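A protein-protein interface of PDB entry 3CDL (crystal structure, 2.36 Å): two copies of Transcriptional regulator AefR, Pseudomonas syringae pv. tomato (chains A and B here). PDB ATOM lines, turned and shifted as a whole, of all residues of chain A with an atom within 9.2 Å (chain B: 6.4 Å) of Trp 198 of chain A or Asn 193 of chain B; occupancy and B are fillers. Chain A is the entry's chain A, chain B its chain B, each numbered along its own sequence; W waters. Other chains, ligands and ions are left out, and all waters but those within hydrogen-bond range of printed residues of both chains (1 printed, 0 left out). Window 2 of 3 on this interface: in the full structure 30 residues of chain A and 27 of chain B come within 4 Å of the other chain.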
ATOM      1  N   ARG A  83      -2.527 -24.864  15.113  1.00  0.00           N
ATOM      2  CA  ARG A  83      -2.148 -23.677  14.356  1.00  0.00           C
ATOM      3  C   ARG A  83      -0.669 -23.567  14.017  1.00  0.00           C
ATOM      4  O   ARG A  83      -0.349 -23.362  12.845  1.00  0.00           O
ATOM      5  CB  ARG A  83      -2.642 -22.388  15.032  1.00  0.00           C
ATOM      6  CG  ARG A  83      -2.906 -21.278  13.998  1.00  0.00           C
ATOM      7  CD  ARG A  83      -3.756 -20.108  14.534  1.00  0.00           C
ATOM      8  NE  ARG A  83      -5.091 -20.557  14.981  1.00  0.00           N
ATOM      9  CZ  ARG A  83      -6.229 -20.219  14.371  1.00  0.00           C
ATOM     10  NH1 ARG A  83      -6.204 -19.390  13.308  1.00  0.00           N
ATOM     11  NH2 ARG A  83      -7.381 -20.707  14.821  1.00  0.00           N
ATOM     12  N   ARG A 146      -8.737 -33.775  17.929  1.00  0.00           N
ATOM     13  CA  ARG A 146      -8.678 -32.315  17.775  1.00  0.00           C
ATOM     14  C   ARG A 146      -9.392 -31.692  16.576  1.00  0.00           C
ATOM     15  O   ARG A 146      -9.476 -30.446  16.494  1.00  0.00           O
ATOM     16  CB  ARG A 146      -7.224 -31.849  17.779  1.00  0.00           C
ATOM     17  CG  ARG A 146      -6.544 -32.002  19.118  1.00  0.00           C
ATOM     18  CD  ARG A 146      -5.071 -31.894  18.946  1.00  0.00           C
ATOM     19  NE  ARG A 146      -4.590 -30.591  19.373  1.00  0.00           N
ATOM     20  CZ  ARG A 146      -3.304 -30.225  19.417  1.00  0.00           C
ATOM     21  NH1 ARG A 146      -2.325 -31.051  19.029  1.00  0.00           N
ATOM     22  NH2 ARG A 146      -2.988 -29.012  19.863  1.00  0.00           N
ATOM     23  N   LEU A 147      -9.840 -32.533  15.639  1.00  0.00           N
ATOM     24  CA  LEU A 147     -10.597 -32.115  14.472  1.00  0.00           C
ATOM     25  C   LEU A 147     -11.882 -32.942  14.341  1.00  0.00           C
ATOM     26  O   LEU A 147     -11.868 -34.151  14.582  1.00  0.00           O
ATOM     27  CB  LEU A 147      -9.765 -32.253  13.194  1.00  0.00           C
ATOM     28  CG  LEU A 147      -8.698 -31.176  12.905  1.00  0.00           C
ATOM     29  CD1 LEU A 147      -7.941 -31.545  11.669  1.00  0.00           C
ATOM     30  CD2 LEU A 147      -9.245 -29.719  12.821  1.00  0.00           C
ATOM     31  N   LYS A 148     -12.982 -32.291  13.963  1.00  0.00           N
ATOM     32  CA  LYS A 148     -14.278 -32.968  13.784  1.00  0.00           C
ATOM     33  C   LYS A 148     -14.168 -34.070  12.727  1.00  0.00           C
ATOM     34  O   LYS A 148     -13.332 -33.975  11.838  1.00  0.00           O
ATOM     35  CB  LYS A 148     -15.363 -31.969  13.385  1.00  0.00           C
ATOM     36  CG  LYS A 148     -15.794 -30.987  14.483  1.00  0.00           C
ATOM     37  CD  LYS A 148     -16.621 -29.814  13.893  1.00  0.00           C
ATOM     38  CE  LYS A 148     -16.978 -28.761  14.976  1.00  0.00           C
ATOM     39  NZ  LYS A 148     -17.575 -27.510  14.354  1.00  0.00           N
ATOM     40  N   PRO A 149     -14.991 -35.143  12.843  1.00  0.00           N
ATOM     41  CA  PRO A 149     -14.972 -36.232  11.855  1.00  0.00           C
ATOM     42  C   PRO A 149     -15.349 -35.730  10.488  1.00  0.00           C
ATOM     43  O   PRO A 149     -16.413 -35.141  10.317  1.00  0.00           O
ATOM     44  CB  PRO A 149     -16.061 -37.194  12.360  1.00  0.00           C
ATOM     45  CG  PRO A 149     -16.922 -36.353  13.270  1.00  0.00           C
ATOM     46  CD  PRO A 149     -15.975 -35.402  13.917  1.00  0.00           C
ATOM     47  N   VAL A 150     -14.484 -35.978   9.514  1.00  0.00           N
ATOM     48  CA  VAL A 150     -14.722 -35.550   8.137  1.00  0.00           C
ATOM     49  C   VAL A 150     -13.825 -36.437   7.273  1.00  0.00           C
ATOM     50  O   VAL A 150     -12.808 -36.944   7.765  1.00  0.00           O
ATOM     51  CB  VAL A 150     -14.410 -33.996   7.941  1.00  0.00           C
ATOM     52  CG1 VAL A 150     -12.935 -33.692   8.130  1.00  0.00           C
ATOM     53  CG2 VAL A 150     -14.903 -33.458   6.597  1.00  0.00           C
ATOM     54  N   PHE A 154     -11.366 -34.860   1.694  1.00  0.00           N
ATOM     55  CA  PHE A 154     -12.310 -33.848   1.333  1.00  0.00           C
ATOM     56  C   PHE A 154     -11.915 -32.548   2.009  1.00  0.00           C
ATOM     57  O   PHE A 154     -12.052 -31.464   1.437  1.00  0.00           O
ATOM     58  CB  PHE A 154     -13.690 -34.314   1.813  1.00  0.00           C
ATOM     59  CG  PHE A 154     -14.751 -33.249   1.815  1.00  0.00           C
ATOM     60  CD1 PHE A 154     -15.758 -33.255   0.838  1.00  0.00           C
ATOM     61  CD2 PHE A 154     -14.790 -32.276   2.812  1.00  0.00           C
ATOM     62  CE1 PHE A 154     -16.752 -32.299   0.826  1.00  0.00           C
ATOM     63  CE2 PHE A 154     -15.795 -31.291   2.798  1.00  0.00           C
ATOM     64  CZ  PHE A 154     -16.780 -31.320   1.812  1.00  0.00           C
ATOM     65  N   ALA A 155     -11.459 -32.661   3.248  1.00  0.00           N
ATOM     66  CA  ALA A 155     -11.103 -31.492   4.009  1.00  0.00           C
ATOM     67  C   ALA A 155      -9.745 -30.981   3.566  1.00  0.00           C
ATOM     68  O   ALA A 155      -9.491 -29.815   3.684  1.00  0.00           O
ATOM     69  CB  ALA A 155     -11.132 -31.779   5.509  1.00  0.00           C
ATOM     70  N   GLN A 158     -10.263 -28.913   0.501  1.00  0.00           N
ATOM     71  CA  GLN A 158     -10.774 -27.574   0.843  1.00  0.00           C
ATOM     72  C   GLN A 158      -9.672 -26.705   1.359  1.00  0.00           C
ATOM     73  O   GLN A 158      -9.643 -25.531   1.078  1.00  0.00           O
ATOM     74  CB  GLN A 158     -11.836 -27.625   1.934  1.00  0.00           C
ATOM     75  CG  GLN A 158     -13.165 -28.121   1.508  1.00  0.00           C
ATOM     76  CD  GLN A 158     -14.093 -28.300   2.690  1.00  0.00           C
ATOM     77  OE1 GLN A 158     -15.292 -27.957   2.625  1.00  0.00           O
ATOM     78  NE2 GLN A 158     -13.553 -28.847   3.790  1.00  0.00           N
ATOM     79  N   LEU A 162      -8.223 -23.036  -0.732  1.00  0.00           N
ATOM     80  CA  LEU A 162      -8.150 -21.723  -0.113  1.00  0.00           C
ATOM     81  C   LEU A 162      -6.811 -21.049  -0.365  1.00  0.00           C
ATOM     82  O   LEU A 162      -6.657 -19.847  -0.149  1.00  0.00           O
ATOM     83  CB  LEU A 162      -8.417 -21.865   1.393  1.00  0.00           C
ATOM     84  CG  LEU A 162      -9.862 -22.117   1.860  1.00  0.00           C
ATOM     85  CD1 LEU A 162      -9.851 -22.098   3.342  1.00  0.00           C
ATOM     86  CD2 LEU A 162     -10.876 -21.113   1.315  1.00  0.00           C
ATOM     87  N   SER A 190      -6.050 -16.388   6.509  1.00  0.00           N
ATOM     88  CA  SER A 190      -7.487 -16.510   6.315  1.00  0.00           C
ATOM     89  C   SER A 190      -7.893 -17.971   6.163  1.00  0.00           C
ATOM     90  O   SER A 190      -8.871 -18.402   6.760  1.00  0.00           O
ATOM     91  CB  SER A 190      -7.947 -15.732   5.101  1.00  0.00           C
ATOM     92  OG  SER A 190      -9.319 -15.438   5.215  1.00  0.00           O
ATOM     93  N   ALA A 191      -7.136 -18.718   5.375  1.00  0.00           N
ATOM     94  CA  ALA A 191      -7.338 -20.148   5.248  1.00  0.00           C
ATOM     95  C   ALA A 191      -7.307 -20.810   6.618  1.00  0.00           C
ATOM     96  O   ALA A 191      -8.184 -21.613   6.949  1.00  0.00           O
ATOM     97  CB  ALA A 191      -6.279 -20.788   4.297  1.00  0.00           C
ATOM     98  N   LEU A 192      -6.298 -20.458   7.412  1.00  0.00           N
ATOM     99  CA  LEU A 192      -6.134 -21.012   8.753  1.00  0.00           C
ATOM    100  C   LEU A 192      -7.345 -20.798   9.637  1.00  0.00           C
ATOM    101  O   LEU A 192      -7.862 -21.729  10.271  1.00  0.00           O
ATOM    102  CB  LEU A 192      -4.953 -20.350   9.427  1.00  0.00           C
ATOM    103  CG  LEU A 192      -3.695 -21.175   9.515  1.00  0.00           C
ATOM    104  CD1 LEU A 192      -2.868 -20.558  10.602  1.00  0.00           C
ATOM    105  CD2 LEU A 192      -4.011 -22.645   9.822  1.00  0.00           C
ATOM    106  N   ASN A 193      -7.771 -19.544   9.682  1.00  0.00           N
ATOM    107  CA  ASN A 193      -8.916 -19.136  10.445  1.00  0.00           C
ATOM    108  C   ASN A 193     -10.172 -19.818  10.006  1.00  0.00           C
ATOM    109  O   ASN A 193     -10.868 -20.387  10.820  1.00  0.00           O
ATOM    110  CB  ASN A 193      -9.055 -17.641  10.350  1.00  0.00           C
ATOM    111  CG  ASN A 193      -8.047 -16.938  11.206  1.00  0.00           C
ATOM    112  OD1 ASN A 193      -7.525 -17.511  12.170  1.00  0.00           O
ATOM    113  ND2 ASN A 193      -7.759 -15.692  10.870  1.00  0.00           N
ATOM    114  N   MET A 194     -10.440 -19.765   8.707  1.00  0.00           N
ATOM    115  CA  MET A 194     -11.564 -20.440   8.074  1.00  0.00           C
ATOM    116  C   MET A 194     -11.581 -21.942   8.346  1.00  0.00           C
ATOM    117  O   MET A 194     -12.608 -22.512   8.753  1.00  0.00           O
ATOM    118  CB  MET A 194     -11.477 -20.229   6.574  1.00  0.00           C
ATOM    119  CG  MET A 194     -12.188 -19.015   6.059  1.00  0.00           C
ATOM    120  SD  MET A 194     -13.208 -19.633   4.517  1.00  0.00           S
ATOM    121  CE  MET A 194     -14.573 -18.277   4.648  1.00  0.00           C
ATOM    122  N   PHE A 195     -10.443 -22.584   8.128  1.00  0.00           N
ATOM    123  CA  PHE A 195     -10.394 -24.014   8.291  1.00  0.00           C
ATOM    124  C   PHE A 195     -10.588 -24.496   9.752  1.00  0.00           C
ATOM    125  O   PHE A 195     -11.359 -25.423  10.021  1.00  0.00           O
ATOM    126  CB  PHE A 195      -9.107 -24.601   7.689  1.00  0.00           C
ATOM    127  CG  PHE A 195      -9.038 -26.089   7.818  1.00  0.00           C
ATOM    128  CD1 PHE A 195      -9.585 -26.914   6.817  1.00  0.00           C
ATOM    129  CD2 PHE A 195      -8.490 -26.677   8.963  1.00  0.00           C
ATOM    130  CE1 PHE A 195      -9.538 -28.295   6.944  1.00  0.00           C
ATOM    131  CE2 PHE A 195      -8.442 -28.072   9.096  1.00  0.00           C
ATOM    132  CZ  PHE A 195      -8.976 -28.881   8.087  1.00  0.00           C
ATOM    133  N   LEU A 196      -9.872 -23.871  10.681  1.00  0.00           N
ATOM    134  CA  LEU A 196      -9.905 -24.294  12.071  1.00  0.00           C
ATOM    135  C   LEU A 196     -11.171 -23.770  12.742  1.00  0.00           C
ATOM    136  O   LEU A 196     -11.833 -24.497  13.491  1.00  0.00           O
ATOM    137  CB  LEU A 196      -8.619 -23.902  12.803  1.00  0.00           C
ATOM    138  CG  LEU A 196      -7.339 -24.654  12.345  1.00  0.00           C
ATOM    139  CD1 LEU A 196      -6.064 -23.962  12.806  1.00  0.00           C
ATOM    140  CD2 LEU A 196      -7.302 -26.120  12.739  1.00  0.00           C
ATOM    141  N   GLY A 197     -11.551 -22.532  12.432  1.00  0.00           N
ATOM    142  CA  GLY A 197     -12.862 -22.044  12.853  1.00  0.00           C
ATOM    143  C   GLY A 197     -13.930 -23.142  12.752  1.00  0.00           C
ATOM    144  O   GLY A 197     -14.585 -23.452  13.743  1.00  0.00           O
ATOM    145  N   TRP A 198     -14.073 -23.757  11.578  1.00  0.00           N
ATOM    146  CA  TRP A 198     -15.052 -24.852  11.364  1.00  0.00           C
ATOM    147  C   TRP A 198     -14.618 -26.237  11.901  1.00  0.00           C
ATOM    148  O   TRP A 198     -15.422 -26.926  12.504  1.00  0.00           O
ATOM    149  CB  TRP A 198     -15.444 -24.965   9.887  1.00  0.00           C
ATOM    150  CG  TRP A 198     -16.430 -26.034   9.601  1.00  0.00           C
ATOM    151  CD1 TRP A 198     -16.222 -27.163   8.840  1.00  0.00           C
ATOM    152  CD2 TRP A 198     -17.811 -26.104  10.046  1.00  0.00           C
ATOM    153  NE1 TRP A 198     -17.375 -27.928   8.803  1.00  0.00           N
ATOM    154  CE2 TRP A 198     -18.357 -27.313   9.535  1.00  0.00           C
ATOM    155  CE3 TRP A 198     -18.625 -25.280  10.836  1.00  0.00           C
ATOM    156  CZ2 TRP A 198     -19.687 -27.711   9.783  1.00  0.00           C
ATOM    157  CZ3 TRP A 198     -19.959 -25.689  11.085  1.00  0.00           C
ATOM    158  CH2 TRP A 198     -20.466 -26.892  10.563  1.00  0.00           C
ATOM    159  N   TYR A 199     -13.369 -26.641  11.701  1.00  0.00           N
ATOM    160  CA  TYR A 199     -13.015 -28.037  11.976  1.00  0.00           C
ATOM    161  C   TYR A 199     -12.473 -28.390  13.354  1.00  0.00           C
ATOM    162  O   TYR A 199     -12.593 -29.563  13.754  1.00  0.00           O
ATOM    163  CB  TYR A 199     -12.042 -28.594  10.924  1.00  0.00           C
ATOM    164  CG  TYR A 199     -12.723 -28.936   9.632  1.00  0.00           C
ATOM    165  CD1 TYR A 199     -13.734 -29.906   9.588  1.00  0.00           C
ATOM    166  CD2 TYR A 199     -12.401 -28.254   8.464  1.00  0.00           C
ATOM    167  CE1 TYR A 199     -14.389 -30.200   8.408  1.00  0.00           C
ATOM    168  CE2 TYR A 199     -13.045 -28.546   7.277  1.00  0.00           C
ATOM    169  CZ  TYR A 199     -14.033 -29.515   7.256  1.00  0.00           C
ATOM    170  OH  TYR A 199     -14.650 -29.783   6.070  1.00  0.00           O
ATOM    171  N   GLU A 200     -11.875 -27.416  14.053  1.00  0.00           N
ATOM    172  CA  GLU A 200     -11.104 -27.697  15.256  1.00  0.00           C
ATOM    173  C   GLU A 200     -12.007 -28.083  16.408  1.00  0.00           C
ATOM    174  O   GLU A 200     -13.057 -27.453  16.620  1.00  0.00           O
ATOM    175  CB  GLU A 200     -10.226 -26.500  15.654  1.00  0.00           C
ATOM    176  CG  GLU A 200      -9.181 -26.861  16.686  1.00  0.00           C
ATOM    177  CD  GLU A 200      -8.229 -25.696  17.122  1.00  0.00           C
ATOM    178  OE1 GLU A 200      -8.413 -24.526  16.705  1.00  0.00           O
ATOM    179  OE2 GLU A 200      -7.284 -25.976  17.912  1.00  0.00           O
ATOM    180  N   ILE A 201     -11.633 -29.134  17.139  1.00  0.00           N
ATOM    181  CA  ILE A 201     -12.227 -29.351  18.470  1.00  0.00           C
ATOM    182  C   ILE A 201     -11.262 -28.779  19.502  1.00  0.00           C
ATOM    183  O   ILE A 201     -10.231 -29.383  19.810  1.00  0.00           O
ATOM    184  CB  ILE A 201     -12.501 -30.810  18.794  1.00  0.00           C
ATOM    185  CG1 ILE A 201     -13.457 -31.414  17.760  1.00  0.00           C
ATOM    186  CG2 ILE A 201     -13.028 -30.937  20.254  1.00  0.00           C
ATOM    187  CD1 ILE A 201     -13.574 -32.939  17.861  1.00  0.00           C
ATOM    188  N   PRO A 202     -11.602 -27.618  20.054  1.00  0.00           N
ATOM    189  CA  PRO A 202     -10.604 -26.872  20.822  1.00  0.00           C
ATOM    190  C   PRO A 202     -10.239 -27.562  22.122  1.00  0.00           C
ATOM    191  O   PRO A 202      -9.055 -27.634  22.440  1.00  0.00           O
ATOM    192  CB  PRO A 202     -11.289 -25.514  21.083  1.00  0.00           C
ATOM    193  CG  PRO A 202     -12.489 -25.463  20.064  1.00  0.00           C
ATOM    194  CD  PRO A 202     -12.906 -26.928  20.002  1.00  0.00           C
ATOM    195  N   ARG B  83     -27.822 -17.726   5.838  1.00  0.00           N
ATOM    196  CA  ARG B  83     -27.785 -19.136   5.514  1.00  0.00           C
ATOM    197  C   ARG B  83     -28.725 -19.462   4.347  1.00  0.00           C
ATOM    198  O   ARG B  83     -28.275 -19.898   3.283  1.00  0.00           O
ATOM    199  CB  ARG B  83     -28.150 -19.949   6.760  1.00  0.00           C
ATOM    200  CG  ARG B  83     -28.052 -21.435   6.568  1.00  0.00           C
ATOM    201  CD  ARG B  83     -28.035 -22.155   7.887  1.00  0.00           C
ATOM    202  NE  ARG B  83     -27.383 -23.449   7.712  1.00  0.00           N
ATOM    203  CZ  ARG B  83     -26.131 -23.727   8.068  1.00  0.00           C
ATOM    204  NH1 ARG B  83     -25.661 -24.941   7.840  1.00  0.00           N
ATOM    205  NH2 ARG B  83     -25.357 -22.813   8.656  1.00  0.00           N
ATOM    206  N   VAL B 188     -21.565 -28.026  -1.115  1.00  0.00           N
ATOM    207  CA  VAL B 188     -22.237 -26.753  -0.863  1.00  0.00           C
ATOM    208  C   VAL B 188     -22.350 -26.488   0.643  1.00  0.00           C
ATOM    209  O   VAL B 188     -21.938 -25.437   1.145  1.00  0.00           O
ATOM    210  CB  VAL B 188     -23.652 -26.712  -1.464  1.00  0.00           C
ATOM    211  CG1 VAL B 188     -24.350 -25.439  -1.054  1.00  0.00           C
ATOM    212  CG2 VAL B 188     -23.594 -26.804  -2.965  1.00  0.00           C
ATOM    213  N   GLU B 189     -22.905 -27.476   1.339  1.00  0.00           N
ATOM    214  CA  GLU B 189     -23.172 -27.426   2.766  1.00  0.00           C
ATOM    215  C   GLU B 189     -21.936 -27.061   3.584  1.00  0.00           C
ATOM    216  O   GLU B 189     -22.002 -26.101   4.357  1.00  0.00           O
ATOM    217  CB  GLU B 189     -23.731 -28.768   3.218  1.00  0.00           C
ATOM    218  CG  GLU B 189     -24.811 -28.662   4.252  1.00  0.00           C
ATOM    219  CD  GLU B 189     -26.203 -28.661   3.647  1.00  0.00           C
ATOM    220  OE1 GLU B 189     -26.670 -29.736   3.195  1.00  0.00           O
ATOM    221  OE2 GLU B 189     -26.842 -27.589   3.656  1.00  0.00           O
ATOM    222  N   SER B 190     -20.825 -27.794   3.423  1.00  0.00           N
ATOM    223  CA  SER B 190     -19.607 -27.418   4.147  1.00  0.00           C
ATOM    224  C   SER B 190     -19.033 -26.094   3.727  1.00  0.00           C
ATOM    225  O   SER B 190     -18.494 -25.386   4.566  1.00  0.00           O
ATOM    226  CB  SER B 190     -18.490 -28.481   4.169  1.00  0.00           C
ATOM    227  OG  SER B 190     -18.435 -29.161   2.947  1.00  0.00           O
ATOM    228  N   ALA B 191     -19.160 -25.746   2.451  1.00  0.00           N
ATOM    229  CA  ALA B 191     -18.707 -24.431   1.980  1.00  0.00           C
ATOM    230  C   ALA B 191     -19.419 -23.379   2.775  1.00  0.00           C
ATOM    231  O   ALA B 191     -18.758 -22.570   3.431  1.00  0.00           O
ATOM    232  CB  ALA B 191     -18.948 -24.256   0.498  1.00  0.00           C
ATOM    233  N   LEU B 192     -20.759 -23.445   2.753  1.00  0.00           N
ATOM    234  CA  LEU B 192     -21.677 -22.597   3.524  1.00  0.00           C
ATOM    235  C   LEU B 192     -21.268 -22.500   4.986  1.00  0.00           C
ATOM    236  O   LEU B 192     -21.052 -21.400   5.520  1.00  0.00           O
ATOM    237  CB  LEU B 192     -23.102 -23.181   3.453  1.00  0.00           C
ATOM    238  CG  LEU B 192     -24.410 -22.361   3.539  1.00  0.00           C
ATOM    239  CD1 LEU B 192     -25.564 -23.191   4.126  1.00  0.00           C
ATOM    240  CD2 LEU B 192     -24.286 -21.096   4.315  1.00  0.00           C
ATOM    241  N   ASN B 193     -21.189 -23.668   5.628  1.00  0.00           N
ATOM    242  CA  ASN B 193     -20.853 -23.791   7.049  1.00  0.00           C
ATOM    243  C   ASN B 193     -19.490 -23.204   7.362  1.00  0.00           C
ATOM    244  O   ASN B 193     -19.313 -22.503   8.353  1.00  0.00           O
ATOM    245  CB  ASN B 193     -20.894 -25.257   7.482  1.00  0.00           C
ATOM    246  CG  ASN B 193     -22.309 -25.742   7.767  1.00  0.00           C
ATOM    247  OD1 ASN B 193     -23.125 -25.006   8.313  1.00  0.00           O
ATOM    248  ND2 ASN B 193     -22.603 -26.991   7.395  1.00  0.00           N
ATOM    249  N   MET B 194     -18.526 -23.495   6.510  1.00  0.00           N
ATOM    250  CA  MET B 194     -17.193 -22.979   6.700  1.00  0.00           C
ATOM    251  C   MET B 194     -17.204 -21.468   6.511  1.00  0.00           C
ATOM    252  O   MET B 194     -16.663 -20.739   7.330  1.00  0.00           O
ATOM    253  CB  MET B 194     -16.223 -23.632   5.723  1.00  0.00           C
ATOM    254  CG  MET B 194     -14.819 -23.101   5.853  1.00  0.00           C
ATOM    255  SD  MET B 194     -13.533 -24.339   5.170  1.00  0.00           S
ATOM    256  CE  MET B 194     -14.681 -25.925   5.214  1.00  0.00           C
ATOM    257  N   PHE B 195     -17.844 -21.021   5.434  1.00  0.00           N
ATOM    258  CA  PHE B 195     -17.835 -19.610   5.078  1.00  0.00           C
ATOM    259  C   PHE B 195     -18.511 -18.806   6.176  1.00  0.00           C
ATOM    260  O   PHE B 195     -17.901 -17.912   6.775  1.00  0.00           O
ATOM    261  CB  PHE B 195     -18.469 -19.330   3.692  1.00  0.00           C
ATOM    262  CG  PHE B 195     -18.328 -17.882   3.256  1.00  0.00           C
ATOM    263  CD1 PHE B 195     -17.152 -17.435   2.632  1.00  0.00           C
ATOM    264  CD2 PHE B 195     -19.328 -16.950   3.542  1.00  0.00           C
ATOM    265  CE1 PHE B 195     -16.997 -16.095   2.273  1.00  0.00           C
ATOM    266  CE2 PHE B 195     -19.178 -15.601   3.191  1.00  0.00           C
ATOM    267  CZ  PHE B 195     -18.015 -15.173   2.548  1.00  0.00           C
ATOM    268  N   LEU B 196     -19.761 -19.150   6.464  1.00  0.00           N
ATOM    269  CA  LEU B 196     -20.527 -18.340   7.406  1.00  0.00           C
ATOM    270  C   LEU B 196     -19.982 -18.457   8.811  1.00  0.00           C
ATOM    271  O   LEU B 196     -19.992 -17.467   9.563  1.00  0.00           O
ATOM    272  CB  LEU B 196     -22.025 -18.670   7.361  1.00  0.00           C
ATOM    273  CG  LEU B 196     -22.749 -17.884   6.275  1.00  0.00           C
ATOM    274  CD1 LEU B 196     -24.220 -18.163   6.334  1.00  0.00           C
ATOM    275  CD2 LEU B 196     -22.481 -16.392   6.442  1.00  0.00           C
ATOM    276  N   GLY B 197     -19.494 -19.667   9.136  1.00  0.00           N
ATOM    277  CA  GLY B 197     -18.762 -19.942  10.369  1.00  0.00           C
ATOM    278  C   GLY B 197     -17.768 -18.842  10.709  1.00  0.00           C
ATOM    279  O   GLY B 197     -17.739 -18.352  11.845  1.00  0.00           O
ATOM    280  N   TRP B 198     -16.967 -18.439   9.715  1.00  0.00           N
ATOM    281  CA  TRP B 198     -15.902 -17.447   9.912  1.00  0.00           C
ATOM    282  C   TRP B 198     -16.361 -16.011   9.718  1.00  0.00           C
ATOM    283  O   TRP B 198     -16.005 -15.137  10.494  1.00  0.00           O
ATOM    284  CB  TRP B 198     -14.679 -17.748   9.020  1.00  0.00           C
ATOM    285  CG  TRP B 198     -13.614 -16.688   9.140  1.00  0.00           C
ATOM    286  CD1 TRP B 198     -13.244 -15.805   8.177  1.00  0.00           C
ATOM    287  CD2 TRP B 198     -12.818 -16.372  10.300  1.00  0.00           C
ATOM    288  NE1 TRP B 198     -12.264 -14.959   8.649  1.00  0.00           N
ATOM    289  CE2 TRP B 198     -11.983 -15.284   9.951  1.00  0.00           C
ATOM    290  CE3 TRP B 198     -12.738 -16.892  11.603  1.00  0.00           C
ATOM    291  CZ2 TRP B 198     -11.067 -14.709  10.856  1.00  0.00           C
ATOM    292  CZ3 TRP B 198     -11.824 -16.316  12.506  1.00  0.00           C
ATOM    293  CH2 TRP B 198     -11.001 -15.242  12.120  1.00  0.00           C
HETATM  294  O   HOH W   1     -14.873 -21.305   9.658  1.00  0.00           O
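The side-chain hydroxyl of Ser 190 of chain B is in hydrogen-bond range of the side-chain amide oxygen of Gln 158 of chain A, at 3.4 Å.
NE2 of Gln 158 of chain A sits at hydrogen-bond distance from OH of Tyr 199 of chain A. OD1 of Asn 193 of chain B lies within hydrogen-bond range of NH1 of Arg 83 of chain B (2.6 Å). O of Glu 189 of chain B lies within hydrogen-bond range of ND2 of Asn 193 of chain B, at 3.2 Å. O of Trp 198 of chain A lies within hydrogen-bond range of NZ of Lys 148 of chain A. The guanidinium group (NH1) of Arg 83 of chain A sits at hydrogen-bond distance from the side-chain amide oxygen (OD1) of Asn 193 of chain A. O of Tyr 199 of chain A sits at hydrogen-bond distance from N of Lys 148 of chain A (2.8 Å).
OG of Ser 190 of chain B touches CZ of Phe 154 of chain A, 2.9 Å away. OE1 of Gln 158 of chain A touches CE of Met 194 of chain B (3.3 Å). Trp 198 of chain B touches Asn 193 of chain A. Met 194 of chain B touches Met 194 of chain A (CG to O, 3.7 Å). Met 194 of chain A touches Phe 195 of chain B (CE to CD1, 3.4 Å). Met 194 of chain A touches Trp 198 of chain B. Asn 193 of chain B touches Trp 198 of chain A (CB to CH2, 3.5 Å). Tyr 199 of chain A touches Met 194 of chain B (CE2 to CE, 3.7 Å).
Ala 155 of chain A touches none of the printed residues of chain B. Of the printed residues of chain B, Tyr 199 of chain A touches Met 194 (3.7 Å). Printed residues of chain A within 4 Å of Ser 190 of chain B: Phe 154 (2.9 Å) and Gln 158 (3.4 Å). No residue of chain A comes within 4 Å of Leu 192 of chain B. Asn 193 of chain B touches just one residue of chain A: Trp 198. Printed residues of chain A within 4 Å of Phe 195 of chain B: Met 194. The nearest residue of chain B that does not touch Trp 198 of chain A is Met 194 of chain B (4.1 Å). The nearest residue of chain A that does not touch Asn 193 of chain B is Met 194 of chain A (6.7 Å).
Of the 12 printed residues of chain B, 5 touch a printed residue of chain A. Of the 23 printed residues of chain A, 6 touch a printed residue of chain B. Hydrophobic or aromatic side chains of chain A that line the printed part of chain B: Phe 154, Met 194, Trp 198 and Tyr 199. Among the printed residues, 9 pairs touch across the chains.
Asn 193 of chain A touches Trp 198 of chain B, and with the chains exchanged Trp 198 of chain A touches Asn 193 of chain B. Met 194 of chain B touches its own counterpart, Met 194 of chain A. Met 194 of chain A touches Phe 195 of chain B, but with the chains exchanged Phe 195 of chain A does not touch Met 194 of chain B (4.4 Å). Met 194 of chain A touches Trp 198 of chain B, but with the chains exchanged Trp 198 of chain A does not touch Met 194 of chain B (4.1 Å). 10 positions are printed for both chains. Of the 9 pairs that touch across the chains among the printed residues, 3 have their exchanged pair printed and touching as well.
Water W1 lies within hydrogen-bond range of O of Met 194 of chain A (2.7 Å), O of Met 194 of chain B (3.0 Å) and N of Trp 198 of chain A (3.2 Å).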
